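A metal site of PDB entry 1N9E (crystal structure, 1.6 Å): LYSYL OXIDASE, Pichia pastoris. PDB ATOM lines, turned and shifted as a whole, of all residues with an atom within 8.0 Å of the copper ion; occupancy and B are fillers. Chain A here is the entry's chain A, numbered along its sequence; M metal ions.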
ATOM      1  N   ALA A 382     -30.612  -8.012  12.562  1.00  0.00           N
ATOM      2  CA  ALA A 382     -29.948  -7.149  11.561  1.00  0.00           C
ATOM      3  C   ALA A 382     -30.505  -7.621  10.231  1.00  0.00           C
ATOM      4  O   ALA A 382     -30.218  -8.736   9.783  1.00  0.00           O
ATOM      5  CB  ALA A 382     -28.446  -7.260  11.631  1.00  0.00           C
ATOM      6  N   TYR A 384     -31.033  -6.819   6.289  1.00  0.00           N
ATOM      7  CA  TYR A 384     -30.450  -6.084   5.156  1.00  0.00           C
ATOM      8  C   TYR A 384     -31.398  -5.944   3.980  1.00  0.00           C
ATOM      9  O   TYR A 384     -32.212  -6.819   3.719  1.00  0.00           O
ATOM     10  CB  TYR A 384     -29.164  -6.803   4.703  1.00  0.00           C
ATOM     11  CG  TYR A 384     -28.117  -6.605   5.760  1.00  0.00           C
ATOM     12  CD1 TYR A 384     -28.190  -7.281   6.962  1.00  0.00           C
ATOM     13  CD2 TYR A 384     -27.051  -5.718   5.557  1.00  0.00           C
ATOM     14  CE1 TYR A 384     -27.227  -7.105   7.964  1.00  0.00           C
ATOM     15  CE2 TYR A 384     -26.073  -5.533   6.550  1.00  0.00           C
ATOM     16  CZ  TYR A 384     -26.185  -6.234   7.750  1.00  0.00           C
ATOM     17  OH  TYR A 384     -25.253  -6.078   8.745  1.00  0.00           O
ATOM     18  N   ASN A 477     -18.439  -9.646  12.894  1.00  0.00           N
ATOM     19  CA  ASN A 477     -18.042  -8.279  12.528  1.00  0.00           C
ATOM     20  C   ASN A 477     -18.555  -7.204  13.481  1.00  0.00           C
ATOM     21  O   ASN A 477     -17.928  -6.141  13.563  1.00  0.00           O
ATOM     22  CB  ASN A 477     -18.496  -7.965  11.086  1.00  0.00           C
ATOM     23  CG  ASN A 477     -19.986  -8.269  10.871  1.00  0.00           C
ATOM     24  OD1 ASN A 477     -20.422  -9.410  11.038  1.00  0.00           O
ATOM     25  ND2 ASN A 477     -20.761  -7.256  10.496  1.00  0.00           N
ATOM     26  N   TPQ A 478     -19.737  -7.353  14.166  1.00  0.00           N
ATOM     27  CA  TPQ A 478     -20.369  -6.237  14.889  1.00  0.00           C
ATOM     28  CB  TPQ A 478     -21.915  -6.147  14.832  1.00  0.00           C
ATOM     29  C   TPQ A 478     -19.912  -6.251  16.343  1.00  0.00           C
ATOM     30  O   TPQ A 478     -19.812  -7.329  16.936  1.00  0.00           O
ATOM     31  C1  TPQ A 478     -22.336  -5.150  13.742  1.00  0.00           C
ATOM     32  C2  TPQ A 478     -22.812  -5.670  12.438  1.00  0.00           C
ATOM     33  O2  TPQ A 478     -22.870  -6.897  12.262  1.00  0.00           O
ATOM     34  C3  TPQ A 478     -23.227  -4.728  11.349  1.00  0.00           C
ATOM     35  C4  TPQ A 478     -23.165  -3.356  11.565  1.00  0.00           C
ATOM     36  O4  TPQ A 478     -23.498  -2.549  10.682  1.00  0.00           O
ATOM     37  C5  TPQ A 478     -22.678  -2.827  12.851  1.00  0.00           C
ATOM     38  O5  TPQ A 478     -22.633  -1.567  13.016  1.00  0.00           O
ATOM     39  C6  TPQ A 478     -22.273  -3.781  13.933  1.00  0.00           C
ATOM     40  N   TYR A 480     -21.476  -4.844  19.916  1.00  0.00           N
ATOM     41  CA  TYR A 480     -22.619  -4.209  20.553  1.00  0.00           C
ATOM     42  C   TYR A 480     -22.309  -3.844  21.995  1.00  0.00           C
ATOM     43  O   TYR A 480     -21.904  -4.701  22.776  1.00  0.00           O
ATOM     44  CB  TYR A 480     -23.833  -5.143  20.523  1.00  0.00           C
ATOM     45  CG  TYR A 480     -24.308  -5.396  19.107  1.00  0.00           C
ATOM     46  CD1 TYR A 480     -25.027  -4.432  18.426  1.00  0.00           C
ATOM     47  CD2 TYR A 480     -24.031  -6.602  18.462  1.00  0.00           C
ATOM     48  CE1 TYR A 480     -25.475  -4.645  17.141  1.00  0.00           C
ATOM     49  CE2 TYR A 480     -24.483  -6.830  17.154  1.00  0.00           C
ATOM     50  CZ  TYR A 480     -25.205  -5.832  16.502  1.00  0.00           C
ATOM     51  OH  TYR A 480     -25.675  -5.985  15.216  1.00  0.00           O
ATOM     52  N   ALA A 498     -23.557   0.743  18.794  1.00  0.00           N
ATOM     53  CA  ALA A 498     -22.990  -0.275  17.922  1.00  0.00           C
ATOM     54  C   ALA A 498     -21.731   0.211  17.192  1.00  0.00           C
ATOM     55  O   ALA A 498     -21.566   1.403  16.921  1.00  0.00           O
ATOM     56  CB  ALA A 498     -24.033  -0.759  16.946  1.00  0.00           C
ATOM     57  N   ALA A 499     -20.841  -0.713  16.878  1.00  0.00           N
ATOM     58  CA  ALA A 499     -19.622  -0.387  16.143  1.00  0.00           C
ATOM     59  C   ALA A 499     -19.106  -1.659  15.488  1.00  0.00           C
ATOM     60  O   ALA A 499     -19.806  -2.663  15.449  1.00  0.00           O
ATOM     61  CB  ALA A 499     -18.558   0.176  17.078  1.00  0.00           C
ATOM     62  N   GLY A 500     -17.886  -1.596  14.983  1.00  0.00           N
ATOM     63  CA  GLY A 500     -17.261  -2.723  14.348  1.00  0.00           C
ATOM     64  C   GLY A 500     -17.275  -2.595  12.834  1.00  0.00           C
ATOM     65  O   GLY A 500     -17.419  -1.496  12.296  1.00  0.00           O
ATOM     66  N   TYR A 501     -17.109  -3.714  12.151  1.00  0.00           N
ATOM     67  CA  TYR A 501     -17.125  -3.729  10.693  1.00  0.00           C
ATOM     68  C   TYR A 501     -18.531  -3.943  10.157  1.00  0.00           C
ATOM     69  O   TYR A 501     -19.231  -4.821  10.639  1.00  0.00           O
ATOM     70  CB  TYR A 501     -16.291  -4.896  10.155  1.00  0.00           C
ATOM     71  CG  TYR A 501     -14.789  -4.683  10.170  1.00  0.00           C
ATOM     72  CD1 TYR A 501     -13.984  -5.370  11.071  1.00  0.00           C
ATOM     73  CD2 TYR A 501     -14.184  -3.804   9.282  1.00  0.00           C
ATOM     74  CE1 TYR A 501     -12.600  -5.183  11.100  1.00  0.00           C
ATOM     75  CE2 TYR A 501     -12.814  -3.606   9.298  1.00  0.00           C
ATOM     76  CZ  TYR A 501     -12.030  -4.301  10.199  1.00  0.00           C
ATOM     77  OH  TYR A 501     -10.663  -4.109  10.228  1.00  0.00           O
ATOM     78  N   ILE A 502     -18.933  -3.151   9.185  1.00  0.00           N
ATOM     79  CA  ILE A 502     -20.235  -3.353   8.596  1.00  0.00           C
ATOM     80  C   ILE A 502     -20.228  -4.554   7.671  1.00  0.00           C
ATOM     81  O   ILE A 502     -19.176  -4.958   7.170  1.00  0.00           O
ATOM     82  CB  ILE A 502     -20.621  -2.119   7.753  1.00  0.00           C
ATOM     83  CG1 ILE A 502     -19.614  -1.902   6.614  1.00  0.00           C
ATOM     84  CG2 ILE A 502     -20.689  -0.885   8.650  1.00  0.00           C
ATOM     85  CD1 ILE A 502     -20.020  -0.713   5.718  1.00  0.00           C
ATOM     86  N   GLN A 503     -21.406  -5.128   7.458  1.00  0.00           N
ATOM     87  CA  GLN A 503     -21.552  -6.110   6.396  1.00  0.00           C
ATOM     88  C   GLN A 503     -21.895  -5.298   5.148  1.00  0.00           C
ATOM     89  O   GLN A 503     -23.066  -4.967   4.863  1.00  0.00           O
ATOM     90  CB  GLN A 503     -22.631  -7.154   6.709  1.00  0.00           C
ATOM     91  CG  GLN A 503     -22.791  -8.186   5.554  1.00  0.00           C
ATOM     92  CD  GLN A 503     -23.724  -9.334   5.927  1.00  0.00           C
ATOM     93  OE1 GLN A 503     -23.609  -9.898   7.007  1.00  0.00           O
ATOM     94  NE2 GLN A 503     -24.635  -9.691   5.012  1.00  0.00           N
ATOM     95  N   SER A 526     -24.203  -1.323   2.206  1.00  0.00           N
ATOM     96  CA  SER A 526     -25.536  -1.928   2.295  1.00  0.00           C
ATOM     97  C   SER A 526     -26.427  -1.431   3.472  1.00  0.00           C
ATOM     98  O   SER A 526     -26.021  -1.336   4.636  1.00  0.00           O
ATOM     99  CB  SER A 526     -25.441  -3.479   2.327  1.00  0.00           C
ATOM    100  OG  SER A 526     -24.997  -4.026   1.089  1.00  0.00           O
ATOM    101  N   PHE A 527     -27.666  -1.129   3.108  1.00  0.00           N
ATOM    102  CA  PHE A 527     -28.641  -0.560   4.035  1.00  0.00           C
ATOM    103  C   PHE A 527     -29.234  -1.660   4.925  1.00  0.00           C
ATOM    104  O   PHE A 527     -29.589  -2.734   4.434  1.00  0.00           O
ATOM    105  CB  PHE A 527     -29.684   0.048   3.113  1.00  0.00           C
ATOM    106  CG  PHE A 527     -30.726   0.827   3.798  1.00  0.00           C
ATOM    107  CD1 PHE A 527     -31.990   0.903   3.194  1.00  0.00           C
ATOM    108  CD2 PHE A 527     -30.518   1.479   4.994  1.00  0.00           C
ATOM    109  CE1 PHE A 527     -33.026   1.618   3.783  1.00  0.00           C
ATOM    110  CE2 PHE A 527     -31.557   2.203   5.587  1.00  0.00           C
ATOM    111  CZ  PHE A 527     -32.810   2.275   4.975  1.00  0.00           C
ATOM    112  N   HIS A 528     -29.338  -1.417   6.226  1.00  0.00           N
ATOM    113  CA  HIS A 528     -29.927  -2.416   7.089  1.00  0.00           C
ATOM    114  C   HIS A 528     -30.557  -1.771   8.305  1.00  0.00           C
ATOM    115  O   HIS A 528     -30.201  -0.669   8.690  1.00  0.00           O
ATOM    116  CB  HIS A 528     -28.862  -3.444   7.548  1.00  0.00           C
ATOM    117  CG  HIS A 528     -27.668  -2.831   8.224  1.00  0.00           C
ATOM    118  ND1 HIS A 528     -26.630  -2.276   7.516  1.00  0.00           N
ATOM    119  CD2 HIS A 528     -27.364  -2.679   9.535  1.00  0.00           C
ATOM    120  CE1 HIS A 528     -25.721  -1.804   8.362  1.00  0.00           C
ATOM    121  NE2 HIS A 528     -26.142  -2.045   9.594  1.00  0.00           N
ATOM    122  N   ASP A 529     -31.508  -2.495   8.886  1.00  0.00           N
ATOM    123  CA  ASP A 529     -31.964  -2.138  10.204  1.00  0.00           C
ATOM    124  C   ASP A 529     -31.375  -2.994  11.322  1.00  0.00           C
ATOM    125  O   ASP A 529     -31.258  -4.222  11.200  1.00  0.00           O
ATOM    126  CB  ASP A 529     -33.483  -2.375  10.270  1.00  0.00           C
ATOM    127  CG  ASP A 529     -34.282  -1.300   9.606  1.00  0.00           C
ATOM    128  OD1 ASP A 529     -33.764  -0.172   9.432  1.00  0.00           O
ATOM    129  OD2 ASP A 529     -35.455  -1.495   9.221  1.00  0.00           O
ATOM    130  N   HIS A 530     -31.003  -2.353  12.434  1.00  0.00           N
ATOM    131  CA  HIS A 530     -30.719  -3.088  13.658  1.00  0.00           C
ATOM    132  C   HIS A 530     -31.953  -2.863  14.532  1.00  0.00           C
ATOM    133  O   HIS A 530     -32.403  -1.736  14.693  1.00  0.00           O
ATOM    134  CB  HIS A 530     -29.540  -2.488  14.451  1.00  0.00           C
ATOM    135  CG  HIS A 530     -28.209  -2.585  13.757  1.00  0.00           C
ATOM    136  ND1 HIS A 530     -27.407  -3.695  13.838  1.00  0.00           N
ATOM    137  CD2 HIS A 530     -27.537  -1.694  12.995  1.00  0.00           C
ATOM    138  CE1 HIS A 530     -26.308  -3.505  13.140  1.00  0.00           C
ATOM    139  NE2 HIS A 530     -26.363  -2.286  12.607  1.00  0.00           N
ATOM    140  N   LEU A 692     -31.769   1.106  14.897  1.00  0.00           N
ATOM    141  CA  LEU A 692     -30.996   1.998  14.045  1.00  0.00           C
ATOM    142  C   LEU A 692     -31.287   1.671  12.583  1.00  0.00           C
ATOM    143  O   LEU A 692     -31.276   0.484  12.211  1.00  0.00           O
ATOM    144  CB  LEU A 692     -29.508   1.771  14.267  1.00  0.00           C
ATOM    145  CG  LEU A 692     -28.977   2.027  15.670  1.00  0.00           C
ATOM    146  CD1 LEU A 692     -27.600   1.387  15.804  1.00  0.00           C
ATOM    147  CD2 LEU A 692     -28.957   3.517  15.952  1.00  0.00           C
ATOM    148  N   HIS A 693     -31.546   2.706  11.764  1.00  0.00           N
ATOM    149  CA  HIS A 693     -31.612   2.505  10.303  1.00  0.00           C
ATOM    150  C   HIS A 693     -30.220   2.904   9.848  1.00  0.00           C
ATOM    151  O   HIS A 693     -29.915   4.096   9.749  1.00  0.00           O
ATOM    152  CB  HIS A 693     -32.612   3.414   9.618  1.00  0.00           C
ATOM    153  CG  HIS A 693     -34.005   3.294  10.169  1.00  0.00           C
ATOM    154  ND1 HIS A 693     -34.668   2.085  10.236  1.00  0.00           N
ATOM    155  CD2 HIS A 693     -34.849   4.226  10.659  1.00  0.00           C
ATOM    156  CE1 HIS A 693     -35.873   2.289  10.764  1.00  0.00           C
ATOM    157  NE2 HIS A 693     -36.006   3.574  11.024  1.00  0.00           N
ATOM    158  N   HIS A 694     -29.379   1.912   9.581  1.00  0.00           N
ATOM    159  CA  HIS A 694     -27.969   2.168   9.325  1.00  0.00           C
ATOM    160  C   HIS A 694     -27.672   2.155   7.830  1.00  0.00           C
ATOM    161  O   HIS A 694     -27.858   1.135   7.174  1.00  0.00           O
ATOM    162  CB  HIS A 694     -27.154   1.091  10.038  1.00  0.00           C
ATOM    163  CG  HIS A 694     -25.690   1.404  10.174  1.00  0.00           C
ATOM    164  ND1 HIS A 694     -24.773   0.478  10.635  1.00  0.00           N
ATOM    165  CD2 HIS A 694     -24.985   2.536   9.926  1.00  0.00           C
ATOM    166  CE1 HIS A 694     -23.572   1.027  10.662  1.00  0.00           C
ATOM    167  NE2 HIS A 694     -23.671   2.271  10.233  1.00  0.00           N
ATOM    168  N   LEU A 695     -27.224   3.297   7.330  1.00  0.00           N
ATOM    169  CA  LEU A 695     -26.842   3.476   5.947  1.00  0.00           C
ATOM    170  C   LEU A 695     -25.395   3.926   5.967  1.00  0.00           C
ATOM    171  O   LEU A 695     -25.114   5.125   5.946  1.00  0.00           O
ATOM    172  CB  LEU A 695     -27.696   4.572   5.298  1.00  0.00           C
ATOM    173  CG  LEU A 695     -27.406   4.794   3.800  1.00  0.00           C
ATOM    174  CD1 LEU A 695     -27.931   3.630   2.952  1.00  0.00           C
ATOM    175  CD2 LEU A 695     -28.023   6.105   3.347  1.00  0.00           C
ATOM    176  N   PRO A 696     -24.473   2.973   6.012  1.00  0.00           N
ATOM    177  CA  PRO A 696     -23.072   3.320   6.207  1.00  0.00           C
ATOM    178  C   PRO A 696     -22.501   4.264   5.168  1.00  0.00           C
ATOM    179  O   PRO A 696     -22.883   4.168   4.000  1.00  0.00           O
ATOM    180  CB  PRO A 696     -22.370   1.953   6.152  1.00  0.00           C
ATOM    181  CG  PRO A 696     -23.467   0.985   6.642  1.00  0.00           C
ATOM    182  CD  PRO A 696     -24.676   1.516   5.891  1.00  0.00           C
ATOM    183  N   ASP A 700     -18.072   5.216   8.418  1.00  0.00           N
ATOM    184  CA  ASP A 700     -18.114   3.829   8.885  1.00  0.00           C
ATOM    185  C   ASP A 700     -16.916   3.010   8.405  1.00  0.00           C
ATOM    186  O   ASP A 700     -16.884   1.798   8.617  1.00  0.00           O
ATOM    187  CB  ASP A 700     -19.420   3.154   8.420  1.00  0.00           C
ATOM    188  CG  ASP A 700     -20.628   3.792   9.016  1.00  0.00           C
ATOM    189  OD1 ASP A 700     -21.057   3.370  10.123  1.00  0.00           O
ATOM    190  OD2 ASP A 700     -21.218   4.739   8.451  1.00  0.00           O
ATOM    191  N   THR A 704     -17.534   1.386  12.012  1.00  0.00           N
ATOM    192  CA  THR A 704     -18.597   2.230  12.526  1.00  0.00           C
ATOM    193  C   THR A 704     -18.175   2.763  13.927  1.00  0.00           C
ATOM    194  O   THR A 704     -17.431   2.094  14.654  1.00  0.00           O
ATOM    195  CB  THR A 704     -19.853   1.331  12.636  1.00  0.00           C
ATOM    196  OG1 THR A 704     -20.244   0.953  11.306  1.00  0.00           O
ATOM    197  CG2 THR A 704     -21.056   2.076  13.255  1.00  0.00           C
ATOM    198  N   ALA A 709     -24.030   5.874  16.634  1.00  0.00           N
ATOM    199  CA  ALA A 709     -24.867   4.682  16.420  1.00  0.00           C
ATOM    200  C   ALA A 709     -25.400   4.322  17.807  1.00  0.00           C
ATOM    201  O   ALA A 709     -24.924   3.390  18.436  1.00  0.00           O
ATOM    202  CB  ALA A 709     -24.074   3.530  15.803  1.00  0.00           C
HETATM  203 CU    CU M   1     -25.164  -1.435  11.181  1.00  0.00          CU
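A ring nitrogen (NE2) of His 694 is in hydrogen-bond range of the side-chain carboxylate (OD1) of Asp 700 (2.8 Å).
O2 of TPQ 478 lies within hydrogen-bond range of the side-chain amide nitrogen of Asn 477.
A ring nitrogen (ND1) of His 530 sits at hydrogen-bond distance from the side-chain hydroxyl (OH) of Tyr 480, 3.2 Å away.
A ring nitrogen (ND1) of His 528 sits at hydrogen-bond distance from the backbone carbonyl oxygen of Ser 526 (3.1 Å).
The backbone NH (N) of His 530 is in hydrogen-bond range of the backbone carbonyl oxygen (O) of Leu 692, at 2.9 Å.
Four residues have an atom within 4 Å of the copper ion: TPQ 478, His 528, His 530 and His 694.
The copper ion is bound by NE2 of His 528 (2.0 Å).
ND1 of His 694 binds the copper ion, at 2.0 Å.
NE2 of His 530 binds the copper ion (2.0 Å).
O4 of TPQ 478 binds the copper ion (2.1 Å).
The copper ion has four donor atoms within binding distance.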
